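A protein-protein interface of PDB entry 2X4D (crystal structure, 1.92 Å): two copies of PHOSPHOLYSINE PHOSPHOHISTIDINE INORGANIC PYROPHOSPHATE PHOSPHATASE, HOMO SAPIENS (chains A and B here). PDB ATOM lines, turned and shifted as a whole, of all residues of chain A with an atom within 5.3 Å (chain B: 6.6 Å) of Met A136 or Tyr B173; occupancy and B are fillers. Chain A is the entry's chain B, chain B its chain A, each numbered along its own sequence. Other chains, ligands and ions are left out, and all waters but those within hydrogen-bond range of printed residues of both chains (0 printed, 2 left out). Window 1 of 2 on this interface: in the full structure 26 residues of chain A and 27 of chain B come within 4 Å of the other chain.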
ATOM      1  N   LEU A 102      20.112  -8.523 -38.419  1.00  0.00           N
ATOM      2  CA  LEU A 102      20.309  -9.604 -37.506  1.00  0.00           C
ATOM      3  C   LEU A 102      19.173 -10.568 -37.780  1.00  0.00           C
ATOM      4  O   LEU A 102      18.097 -10.461 -37.192  1.00  0.00           O
ATOM      5  CB  LEU A 102      20.286  -9.041 -36.084  1.00  0.00           C
ATOM      6  CG  LEU A 102      20.655  -9.961 -34.952  1.00  0.00           C
ATOM      7  CD1 LEU A 102      22.036 -10.577 -35.206  1.00  0.00           C
ATOM      8  CD2 LEU A 102      20.586  -9.136 -33.705  1.00  0.00           C
ATOM      9  N   ILE A 124      16.111  -6.637 -36.286  1.00  0.00           N
ATOM     10  CA  ILE A 124      16.242  -7.933 -35.633  1.00  0.00           C
ATOM     11  C   ILE A 124      14.992  -8.777 -35.928  1.00  0.00           C
ATOM     12  O   ILE A 124      13.856  -8.271 -35.902  1.00  0.00           O
ATOM     13  CB  ILE A 124      16.467  -7.755 -34.114  1.00  0.00           C
ATOM     14  CG1 ILE A 124      16.683  -9.102 -33.410  1.00  0.00           C
ATOM     15  CG2 ILE A 124      15.327  -6.991 -33.485  1.00  0.00           C
ATOM     16  CD1 ILE A 124      17.065  -8.951 -31.921  1.00  0.00           C
ATOM     17  N   PHE A 131      21.593 -16.132 -34.100  1.00  0.00           N
ATOM     18  CA  PHE A 131      21.817 -15.380 -32.844  1.00  0.00           C
ATOM     19  C   PHE A 131      23.107 -15.863 -32.129  1.00  0.00           C
ATOM     20  O   PHE A 131      23.125 -16.148 -30.915  1.00  0.00           O
ATOM     21  CB  PHE A 131      20.614 -15.463 -31.896  1.00  0.00           C
ATOM     22  CG  PHE A 131      19.452 -14.548 -32.248  1.00  0.00           C
ATOM     23  CD1 PHE A 131      19.645 -13.201 -32.507  1.00  0.00           C
ATOM     24  CD2 PHE A 131      18.146 -15.041 -32.257  1.00  0.00           C
ATOM     25  CE1 PHE A 131      18.573 -12.367 -32.782  1.00  0.00           C
ATOM     26  CE2 PHE A 131      17.068 -14.214 -32.524  1.00  0.00           C
ATOM     27  CZ  PHE A 131      17.284 -12.877 -32.791  1.00  0.00           C
ATOM     28  N   SER A 132      24.198 -15.896 -32.876  1.00  0.00           N
ATOM     29  CA  SER A 132      25.516 -16.091 -32.307  1.00  0.00           C
ATOM     30  C   SER A 132      25.892 -14.858 -31.462  1.00  0.00           C
ATOM     31  O   SER A 132      25.290 -13.810 -31.597  1.00  0.00           O
ATOM     32  CB  SER A 132      26.536 -16.290 -33.434  1.00  0.00           C
ATOM     33  OG  SER A 132      26.515 -15.186 -34.304  1.00  0.00           O
ATOM     34  N   TYR A 133      26.862 -15.000 -30.574  1.00  0.00           N
ATOM     35  CA  TYR A 133      27.358 -13.864 -29.789  1.00  0.00           C
ATOM     36  C   TYR A 133      28.022 -12.872 -30.745  1.00  0.00           C
ATOM     37  O   TYR A 133      27.787 -11.684 -30.663  1.00  0.00           O
ATOM     38  CB  TYR A 133      28.341 -14.336 -28.716  1.00  0.00           C
ATOM     39  CG  TYR A 133      28.894 -13.229 -27.854  1.00  0.00           C
ATOM     40  CD1 TYR A 133      28.144 -12.694 -26.811  1.00  0.00           C
ATOM     41  CD2 TYR A 133      30.180 -12.729 -28.081  1.00  0.00           C
ATOM     42  CE1 TYR A 133      28.640 -11.672 -26.035  1.00  0.00           C
ATOM     43  CE2 TYR A 133      30.703 -11.709 -27.294  1.00  0.00           C
ATOM     44  CZ  TYR A 133      29.935 -11.192 -26.265  1.00  0.00           C
ATOM     45  OH  TYR A 133      30.460 -10.190 -25.510  1.00  0.00           O
ATOM     46  N   GLN A 134      28.816 -13.371 -31.681  1.00  0.00           N
ATOM     47  CA  GLN A 134      29.417 -12.509 -32.702  1.00  0.00           C
ATOM     48  C   GLN A 134      28.385 -11.634 -33.422  1.00  0.00           C
ATOM     49  O   GLN A 134      28.566 -10.421 -33.535  1.00  0.00           O
ATOM     50  CB  GLN A 134      30.173 -13.338 -33.713  1.00  0.00           C
ATOM     51  CG  GLN A 134      30.577 -12.563 -34.960  1.00  0.00           C
ATOM     52  CD  GLN A 134      31.450 -13.355 -35.898  1.00  0.00           C
ATOM     53  OE1 GLN A 134      30.978 -14.224 -36.631  1.00  0.00           O
ATOM     54  NE2 GLN A 134      32.738 -13.039 -35.897  1.00  0.00           N
ATOM     55  N   ASN A 135      27.298 -12.232 -33.883  1.00  0.00           N
ATOM     56  CA  ASN A 135      26.279 -11.457 -34.594  1.00  0.00           C
ATOM     57  C   ASN A 135      25.546 -10.471 -33.705  1.00  0.00           C
ATOM     58  O   ASN A 135      25.292  -9.358 -34.108  1.00  0.00           O
ATOM     59  CB  ASN A 135      25.280 -12.375 -35.288  1.00  0.00           C
ATOM     60  CG  ASN A 135      25.865 -13.035 -36.520  1.00  0.00           C
ATOM     61  OD1 ASN A 135      26.916 -12.616 -37.021  1.00  0.00           O
ATOM     62  ND2 ASN A 135      25.220 -14.099 -36.992  1.00  0.00           N
ATOM     63  N   MET A 136      25.203 -10.902 -32.497  1.00  0.00           N
ATOM     64  CA  MET A 136      24.558 -10.037 -31.518  1.00  0.00           C
ATOM     65  C   MET A 136      25.484  -8.904 -31.103  1.00  0.00           C
ATOM     66  O   MET A 136      25.063  -7.747 -31.023  1.00  0.00           O
ATOM     67  CB  MET A 136      24.120 -10.830 -30.294  1.00  0.00           C
ATOM     68  CG  MET A 136      22.805 -11.577 -30.493  1.00  0.00           C
ATOM     69  SD  MET A 136      21.406 -10.458 -30.359  1.00  0.00           S
ATOM     70  CE  MET A 136      21.464 -10.113 -28.573  1.00  0.00           C
ATOM     71  N   ASN A 137      26.742  -9.237 -30.844  1.00  0.00           N
ATOM     72  CA  ASN A 137      27.707  -8.225 -30.481  1.00  0.00           C
ATOM     73  C   ASN A 137      27.940  -7.219 -31.582  1.00  0.00           C
ATOM     74  O   ASN A 137      28.086  -6.059 -31.306  1.00  0.00           O
ATOM     75  CB  ASN A 137      29.063  -8.836 -30.068  1.00  0.00           C
ATOM     76  CG  ASN A 137      29.826  -7.936 -29.117  1.00  0.00           C
ATOM     77  OD1 ASN A 137      29.317  -7.581 -28.055  1.00  0.00           O
ATOM     78  ND2 ASN A 137      31.011  -7.511 -29.518  1.00  0.00           N
ATOM     79  N   ASN A 138      27.971  -7.669 -32.829  1.00  0.00           N
ATOM     80  CA  ASN A 138      28.141  -6.760 -33.960  1.00  0.00           C
ATOM     81  C   ASN A 138      26.968  -5.797 -34.111  1.00  0.00           C
ATOM     82  O   ASN A 138      27.169  -4.633 -34.393  1.00  0.00           O
ATOM     83  CB  ASN A 138      28.321  -7.526 -35.278  1.00  0.00           C
ATOM     84  CG  ASN A 138      29.703  -8.172 -35.419  1.00  0.00           C
ATOM     85  OD1 ASN A 138      30.642  -7.801 -34.739  1.00  0.00           O
ATOM     86  ND2 ASN A 138      29.812  -9.142 -36.302  1.00  0.00           N
ATOM     87  N   ALA A 139      25.749  -6.297 -33.961  1.00  0.00           N
ATOM     88  CA  ALA A 139      24.544  -5.435 -33.959  1.00  0.00           C
ATOM     89  C   ALA A 139      24.653  -4.396 -32.825  1.00  0.00           C
ATOM     90  O   ALA A 139      24.395  -3.217 -33.051  1.00  0.00           O
ATOM     91  CB  ALA A 139      23.281  -6.254 -33.828  1.00  0.00           C
ATOM     92  N   PHE A 140      25.012  -4.869 -31.627  1.00  0.00           N
ATOM     93  CA  PHE A 140      25.274  -4.038 -30.463  1.00  0.00           C
ATOM     94  C   PHE A 140      26.291  -2.939 -30.708  1.00  0.00           C
ATOM     95  O   PHE A 140      26.081  -1.775 -30.374  1.00  0.00           O
ATOM     96  CB  PHE A 140      25.763  -4.928 -29.293  1.00  0.00           C
ATOM     97  CG  PHE A 140      26.227  -4.157 -28.084  1.00  0.00           C
ATOM     98  CD1 PHE A 140      25.341  -3.355 -27.362  1.00  0.00           C
ATOM     99  CD2 PHE A 140      27.543  -4.282 -27.636  1.00  0.00           C
ATOM    100  CE1 PHE A 140      25.768  -2.663 -26.250  1.00  0.00           C
ATOM    101  CE2 PHE A 140      27.998  -3.578 -26.493  1.00  0.00           C
ATOM    102  CZ  PHE A 140      27.124  -2.771 -25.820  1.00  0.00           C
ATOM    103  N   GLN A 141      27.413  -3.307 -31.311  1.00  0.00           N
ATOM    104  CA  GLN A 141      28.452  -2.333 -31.563  1.00  0.00           C
ATOM    105  C   GLN A 141      28.027  -1.311 -32.643  1.00  0.00           C
ATOM    106  O   GLN A 141      28.384  -0.136 -32.532  1.00  0.00           O
ATOM    107  CB  GLN A 141      29.765  -3.009 -31.940  1.00  0.00           C
ATOM    108  CG  GLN A 141      30.436  -3.713 -30.750  1.00  0.00           C
ATOM    109  CD  GLN A 141      31.818  -4.290 -31.090  1.00  0.00           C
ATOM    110  OE1 GLN A 141      32.145  -4.468 -32.253  1.00  0.00           O
ATOM    111  NE2 GLN A 141      32.632  -4.557 -30.065  1.00  0.00           N
ATOM    112  N   TYR A 173      15.846 -11.660 -27.611  1.00  0.00           N
ATOM    113  CA  TYR A 173      17.008 -11.002 -28.193  1.00  0.00           C
ATOM    114  C   TYR A 173      16.764  -9.507 -28.438  1.00  0.00           C
ATOM    115  O   TYR A 173      17.690  -8.700 -28.281  1.00  0.00           O
ATOM    116  CB  TYR A 173      17.436 -11.731 -29.474  1.00  0.00           C
ATOM    117  CG  TYR A 173      17.965 -13.113 -29.146  1.00  0.00           C
ATOM    118  CD1 TYR A 173      19.312 -13.303 -28.811  1.00  0.00           C
ATOM    119  CD2 TYR A 173      17.118 -14.201 -29.077  1.00  0.00           C
ATOM    120  CE1 TYR A 173      19.802 -14.563 -28.469  1.00  0.00           C
ATOM    121  CE2 TYR A 173      17.593 -15.458 -28.748  1.00  0.00           C
ATOM    122  CZ  TYR A 173      18.924 -15.645 -28.455  1.00  0.00           C
ATOM    123  OH  TYR A 173      19.388 -16.894 -28.123  1.00  0.00           O
ATOM    124  N   ALA A 176      17.314  -8.044 -24.999  1.00  0.00           N
ATOM    125  CA  ALA A 176      18.736  -8.003 -24.745  1.00  0.00           C
ATOM    126  C   ALA A 176      19.357  -6.711 -25.292  1.00  0.00           C
ATOM    127  O   ALA A 176      19.997  -5.968 -24.552  1.00  0.00           O
ATOM    128  CB  ALA A 176      19.410  -9.229 -25.313  1.00  0.00           C
ATOM    129  N   LEU A 177      19.134  -6.416 -26.573  1.00  0.00           N
ATOM    130  CA  LEU A 177      19.649  -5.162 -27.125  1.00  0.00           C
ATOM    131  C   LEU A 177      19.037  -3.909 -26.492  1.00  0.00           C
ATOM    132  O   LEU A 177      19.732  -2.941 -26.272  1.00  0.00           O
ATOM    133  CB  LEU A 177      19.497  -5.114 -28.628  1.00  0.00           C
ATOM    134  CG  LEU A 177      20.255  -6.168 -29.451  1.00  0.00           C
ATOM    135  CD1 LEU A 177      20.021  -5.944 -31.000  1.00  0.00           C
ATOM    136  CD2 LEU A 177      21.733  -6.219 -29.126  1.00  0.00           C
ATOM    137  N   LEU B 102      25.156 -21.819 -17.940  1.00  0.00           N
ATOM    138  CA  LEU B 102      25.280 -21.049 -19.157  1.00  0.00           C
ATOM    139  C   LEU B 102      26.493 -20.121 -18.964  1.00  0.00           C
ATOM    140  O   LEU B 102      26.377 -18.969 -18.496  1.00  0.00           O
ATOM    141  CB  LEU B 102      23.966 -20.316 -19.416  1.00  0.00           C
ATOM    142  CG  LEU B 102      23.809 -19.585 -20.732  1.00  0.00           C
ATOM    143  CD1 LEU B 102      24.082 -20.483 -21.965  1.00  0.00           C
ATOM    144  CD2 LEU B 102      22.394 -18.991 -20.765  1.00  0.00           C
ATOM    145  N   ILE B 124      23.540 -18.199 -15.096  1.00  0.00           N
ATOM    146  CA  ILE B 124      24.028 -17.470 -16.273  1.00  0.00           C
ATOM    147  C   ILE B 124      25.179 -16.543 -15.847  1.00  0.00           C
ATOM    148  O   ILE B 124      25.126 -15.874 -14.791  1.00  0.00           O
ATOM    149  CB  ILE B 124      22.875 -16.668 -16.960  1.00  0.00           C
ATOM    150  CG1 ILE B 124      23.332 -16.010 -18.254  1.00  0.00           C
ATOM    151  CG2 ILE B 124      22.267 -15.611 -16.048  1.00  0.00           C
ATOM    152  CD1 ILE B 124      22.175 -15.386 -19.067  1.00  0.00           C
ATOM    153  N   ALA B 125      26.232 -16.537 -16.654  1.00  0.00           N
ATOM    154  CA  ALA B 125      27.401 -15.749 -16.342  1.00  0.00           C
ATOM    155  C   ALA B 125      27.825 -15.047 -17.621  1.00  0.00           C
ATOM    156  O   ALA B 125      27.074 -15.050 -18.587  1.00  0.00           O
ATOM    157  CB  ALA B 125      28.523 -16.657 -15.757  1.00  0.00           C
ATOM    158  N   GLY B 128      30.089 -14.980 -23.156  1.00  0.00           N
ATOM    159  CA  GLY B 128      30.678 -14.593 -24.447  1.00  0.00           C
ATOM    160  C   GLY B 128      30.270 -15.502 -25.584  1.00  0.00           C
ATOM    161  O   GLY B 128      29.077 -15.705 -25.834  1.00  0.00           O
ATOM    162  N   PHE B 131      27.384 -17.945 -25.485  1.00  0.00           N
ATOM    163  CA  PHE B 131      25.985 -17.537 -25.713  1.00  0.00           C
ATOM    164  C   PHE B 131      25.494 -17.877 -27.156  1.00  0.00           C
ATOM    165  O   PHE B 131      24.915 -17.037 -27.885  1.00  0.00           O
ATOM    166  CB  PHE B 131      25.787 -16.046 -25.425  1.00  0.00           C
ATOM    167  CG  PHE B 131      25.674 -15.696 -23.954  1.00  0.00           C
ATOM    168  CD1 PHE B 131      24.814 -16.381 -23.127  1.00  0.00           C
ATOM    169  CD2 PHE B 131      26.416 -14.643 -23.421  1.00  0.00           C
ATOM    170  CE1 PHE B 131      24.708 -16.061 -21.757  1.00  0.00           C
ATOM    171  CE2 PHE B 131      26.278 -14.275 -22.090  1.00  0.00           C
ATOM    172  CZ  PHE B 131      25.439 -15.004 -21.240  1.00  0.00           C
ATOM    173  N   SER B 132      25.716 -19.119 -27.569  1.00  0.00           N
ATOM    174  CA  SER B 132      25.142 -19.626 -28.805  1.00  0.00           C
ATOM    175  C   SER B 132      23.616 -19.702 -28.644  1.00  0.00           C
ATOM    176  O   SER B 132      23.100 -19.723 -27.533  1.00  0.00           O
ATOM    177  CB  SER B 132      25.713 -21.027 -29.101  1.00  0.00           C
ATOM    178  OG  SER B 132      25.496 -21.869 -27.986  1.00  0.00           O
ATOM    179  N   MET B 136      21.646 -21.070 -25.211  1.00  0.00           N
ATOM    180  CA  MET B 136      20.598 -20.182 -24.698  1.00  0.00           C
ATOM    181  C   MET B 136      19.276 -20.902 -24.747  1.00  0.00           C
ATOM    182  O   MET B 136      18.523 -20.876 -23.774  1.00  0.00           O
ATOM    183  CB  MET B 136      20.505 -18.873 -25.495  1.00  0.00           C
ATOM    184  CG  MET B 136      21.487 -17.803 -25.026  1.00  0.00           C
ATOM    185  SD  MET B 136      20.985 -17.044 -23.474  1.00  0.00           S
ATOM    186  CE  MET B 136      19.489 -16.172 -23.955  1.00  0.00           C
ATOM    187  N   LEU B 151      16.385 -18.632 -11.836  1.00  0.00           N
ATOM    188  CA  LEU B 151      17.463 -18.171 -12.711  1.00  0.00           C
ATOM    189  C   LEU B 151      18.394 -17.360 -11.826  1.00  0.00           C
ATOM    190  O   LEU B 151      17.982 -16.366 -11.242  1.00  0.00           O
ATOM    191  CB  LEU B 151      16.918 -17.303 -13.851  1.00  0.00           C
ATOM    192  CG  LEU B 151      17.945 -16.559 -14.724  1.00  0.00           C
ATOM    193  CD1 LEU B 151      18.901 -17.520 -15.408  1.00  0.00           C
ATOM    194  CD2 LEU B 151      17.263 -15.677 -15.725  1.00  0.00           C
ATOM    195  N   GLY B 157      25.481  -6.773 -15.598  1.00  0.00           N
ATOM    196  CA  GLY B 157      26.125  -5.700 -16.366  1.00  0.00           C
ATOM    197  C   GLY B 157      25.599  -5.690 -17.803  1.00  0.00           C
ATOM    198  O   GLY B 157      25.275  -6.740 -18.336  1.00  0.00           O
ATOM    199  N   LEU B 168      28.956  -7.226 -25.202  1.00  0.00           N
ATOM    200  CA  LEU B 168      27.790  -7.645 -24.439  1.00  0.00           C
ATOM    201  C   LEU B 168      28.133  -8.548 -23.273  1.00  0.00           C
ATOM    202  O   LEU B 168      28.785  -9.613 -23.422  1.00  0.00           O
ATOM    203  CB  LEU B 168      26.801  -8.394 -25.317  1.00  0.00           C
ATOM    204  CG  LEU B 168      26.106  -7.631 -26.428  1.00  0.00           C
ATOM    205  CD1 LEU B 168      25.677  -8.646 -27.450  1.00  0.00           C
ATOM    206  CD2 LEU B 168      24.951  -6.831 -25.866  1.00  0.00           C
ATOM    207  N   ASP B 169      27.647  -8.152 -22.115  1.00  0.00           N
ATOM    208  CA  ASP B 169      27.979  -8.813 -20.844  1.00  0.00           C
ATOM    209  C   ASP B 169      26.853  -9.803 -20.521  1.00  0.00           C
ATOM    210  O   ASP B 169      26.081 -10.166 -21.415  1.00  0.00           O
ATOM    211  CB  ASP B 169      28.117  -7.687 -19.809  1.00  0.00           C
ATOM    212  CG  ASP B 169      28.808  -8.090 -18.512  1.00  0.00           C
ATOM    213  OD1 ASP B 169      29.180  -9.282 -18.273  1.00  0.00           O
ATOM    214  OD2 ASP B 169      28.928  -7.152 -17.680  1.00  0.00           O
ATOM    215  N   VAL B 170      26.750 -10.222 -19.250  1.00  0.00           N
ATOM    216  CA  VAL B 170      25.744 -11.164 -18.807  1.00  0.00           C
ATOM    217  C   VAL B 170      24.325 -10.566 -18.848  1.00  0.00           C
ATOM    218  O   VAL B 170      23.394 -11.251 -19.189  1.00  0.00           O
ATOM    219  CB  VAL B 170      26.076 -11.703 -17.382  1.00  0.00           C
ATOM    220  CG1 VAL B 170      26.072 -10.554 -16.325  1.00  0.00           C
ATOM    221  CG2 VAL B 170      25.152 -12.811 -16.975  1.00  0.00           C
ATOM    222  N   GLY B 171      24.190  -9.294 -18.516  1.00  0.00           N
ATOM    223  CA  GLY B 171      22.881  -8.652 -18.307  1.00  0.00           C
ATOM    224  C   GLY B 171      21.864  -8.800 -19.425  1.00  0.00           C
ATOM    225  O   GLY B 171      20.732  -9.216 -19.182  1.00  0.00           O
ATOM    226  N   PRO B 172      22.267  -8.470 -20.675  1.00  0.00           N
ATOM    227  CA  PRO B 172      21.355  -8.580 -21.788  1.00  0.00           C
ATOM    228  C   PRO B 172      20.784 -10.003 -21.969  1.00  0.00           C
ATOM    229  O   PRO B 172      19.569 -10.156 -22.271  1.00  0.00           O
ATOM    230  CB  PRO B 172      22.224  -8.175 -22.986  1.00  0.00           C
ATOM    231  CG  PRO B 172      23.214  -7.264 -22.410  1.00  0.00           C
ATOM    232  CD  PRO B 172      23.547  -7.868 -21.080  1.00  0.00           C
ATOM    233  N   TYR B 173      21.650 -11.014 -21.770  1.00  0.00           N
ATOM    234  CA  TYR B 173      21.237 -12.429 -21.869  1.00  0.00           C
ATOM    235  C   TYR B 173      20.381 -12.847 -20.674  1.00  0.00           C
ATOM    236  O   TYR B 173      19.477 -13.645 -20.829  1.00  0.00           O
ATOM    237  CB  TYR B 173      22.461 -13.341 -22.082  1.00  0.00           C
ATOM    238  CG  TYR B 173      23.076 -13.087 -23.446  1.00  0.00           C
ATOM    239  CD1 TYR B 173      22.647 -13.783 -24.557  1.00  0.00           C
ATOM    240  CD2 TYR B 173      24.100 -12.130 -23.608  1.00  0.00           C
ATOM    241  CE1 TYR B 173      23.191 -13.535 -25.851  1.00  0.00           C
ATOM    242  CE2 TYR B 173      24.655 -11.874 -24.855  1.00  0.00           C
ATOM    243  CZ  TYR B 173      24.206 -12.579 -25.978  1.00  0.00           C
ATOM    244  OH  TYR B 173      24.734 -12.339 -27.230  1.00  0.00           O
ATOM    245  N   MET B 174      20.673 -12.296 -19.494  1.00  0.00           N
ATOM    246  CA  MET B 174      19.793 -12.430 -18.329  1.00  0.00           C
ATOM    247  C   MET B 174      18.387 -11.888 -18.687  1.00  0.00           C
ATOM    248  O   MET B 174      17.394 -12.581 -18.501  1.00  0.00           O
ATOM    249  CB  MET B 174      20.359 -11.675 -17.118  1.00  0.00           C
ATOM    250  CG  MET B 174      19.478 -11.686 -15.854  1.00  0.00           C
ATOM    251  SD  MET B 174      20.027 -10.471 -14.587  1.00  0.00           S
ATOM    252  CE  MET B 174      19.152  -9.085 -15.320  1.00  0.00           C
ATOM    253  N   LYS B 175      18.322 -10.681 -19.243  1.00  0.00           N
ATOM    254  CA  LYS B 175      17.039 -10.068 -19.597  1.00  0.00           C
ATOM    255  C   LYS B 175      16.240 -10.865 -20.652  1.00  0.00           C
ATOM    256  O   LYS B 175      15.026 -10.949 -20.563  1.00  0.00           O
ATOM    257  CB  LYS B 175      17.243  -8.624 -20.062  1.00  0.00           C
ATOM    258  CG  LYS B 175      17.717  -7.686 -18.964  1.00  0.00           C
ATOM    259  CD  LYS B 175      16.617  -7.388 -17.967  1.00  0.00           C
ATOM    260  CE  LYS B 175      17.064  -6.383 -16.870  1.00  0.00           C
ATOM    261  NZ  LYS B 175      16.091  -6.471 -15.734  1.00  0.00           N
ATOM    262  N   ALA B 176      16.956 -11.466 -21.597  1.00  0.00           N
ATOM    263  CA  ALA B 176      16.384 -12.348 -22.598  1.00  0.00           C
ATOM    264  C   ALA B 176      15.634 -13.496 -21.910  1.00  0.00           C
ATOM    265  O   ALA B 176      14.434 -13.680 -22.154  1.00  0.00           O
ATOM    266  CB  ALA B 176      17.474 -12.869 -23.526  1.00  0.00           C
ATOM    267  N   LEU B 177      16.310 -14.229 -21.014  1.00  0.00           N
ATOM    268  CA  LEU B 177      15.636 -15.352 -20.354  1.00  0.00           C
ATOM    269  C   LEU B 177      14.499 -14.875 -19.465  1.00  0.00           C
ATOM    270  O   LEU B 177      13.452 -15.492 -19.409  1.00  0.00           O
ATOM    271  CB  LEU B 177      16.619 -16.231 -19.586  1.00  0.00           C
ATOM    272  CG  LEU B 177      17.710 -16.922 -20.405  1.00  0.00           C
ATOM    273  CD1 LEU B 177      18.666 -17.727 -19.444  1.00  0.00           C
ATOM    274  CD2 LEU B 177      17.105 -17.811 -21.507  1.00  0.00           C
ATOM    275  N   GLU B 178      14.691 -13.777 -18.758  1.00  0.00           N
ATOM    276  CA  GLU B 178      13.606 -13.239 -17.941  1.00  0.00           C
ATOM    277  C   GLU B 178      12.365 -13.020 -18.775  1.00  0.00           C
ATOM    278  O   GLU B 178      11.253 -13.412 -18.379  1.00  0.00           O
ATOM    279  CB  GLU B 178      13.993 -11.916 -17.289  1.00  0.00           C
ATOM    280  CG  GLU B 178      15.026 -12.013 -16.201  1.00  0.00           C
ATOM    281  CD  GLU B 178      15.193 -10.702 -15.428  1.00  0.00           C
ATOM    282  OE1 GLU B 178      14.938  -9.630 -15.998  1.00  0.00           O
ATOM    283  OE2 GLU B 178      15.551 -10.748 -14.244  1.00  0.00           O
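O of Phe A131 touches O of Phe B131, at 3.6 Å. Gly B128 touches Tyr A133 (O to CG, 3.2 Å). Phe B131 touches Tyr A133 (O to N, 3.9 Å). Tyr B173 touches Tyr A133. CD1 of Leu B168 touches C of Met A136, at 3.7 Å. Tyr B173 touches Met A136 (OH to CB, 3.5 Å). CD2 of Leu B168 touches CG of Phe A140, at 3.7 Å. Tyr A173 touches Met B136 (OH to CB, 3.5 Å). Ala A176 touches Pro B172.
Phe B131 touches its own counterpart, Phe A131. Met A136 touches Tyr B173, and with the chains exchanged Tyr A173 touches Met B136. Of the 11 pairs that touch across the chains among the printed residues, 3 have their exchanged pair printed and touching as well.
The side-chain hydroxyl of Tyr A133 is in hydrogen-bond range of the backbone carbonyl oxygen of Leu B168, 2.7 Å away. The backbone NH (N) of Leu B168 is in hydrogen-bond range of the side-chain amide oxygen (OD1) of Asn A137.
Hydrophobic or aromatic side chains of chain B that line the printed part of chain A: Met B136, Leu B168, Pro B172 and Tyr B173. Of the 16 printed residues of chain A, 7 touch a printed residue of chain B. Printed residues of chain A that touch a printed residue of chain B: Phe A131, Tyr A133, Met A136, Asn A137, Phe A140, Tyr A173 and Ala A176. Hydrophobic or aromatic side chains of chain A within 4 Å of the printed part of chain B: Tyr A133, Met A136, Phe A140, Tyr A173 and Ala A176. Among the printed residues, 11 pairs touch across the chains.
Met A136 touches just these residues of chain B: Leu B168 (3.7 Å) and Tyr B173 (3.5 Å). Tyr B173 touches just these residues of chain A: Tyr A133 and Met A136. Printed residues of chain B within 4 Å of Tyr A173: Met B136 (3.5 Å). Of the printed residues of chain B, Phe A131 touches Phe B131 (3.6 Å).
The side-chain amide nitrogen (NE2) of Gln A141 lies close to the side-chain amide nitrogen (ND2) of Asn A137, 3.4 Å away.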
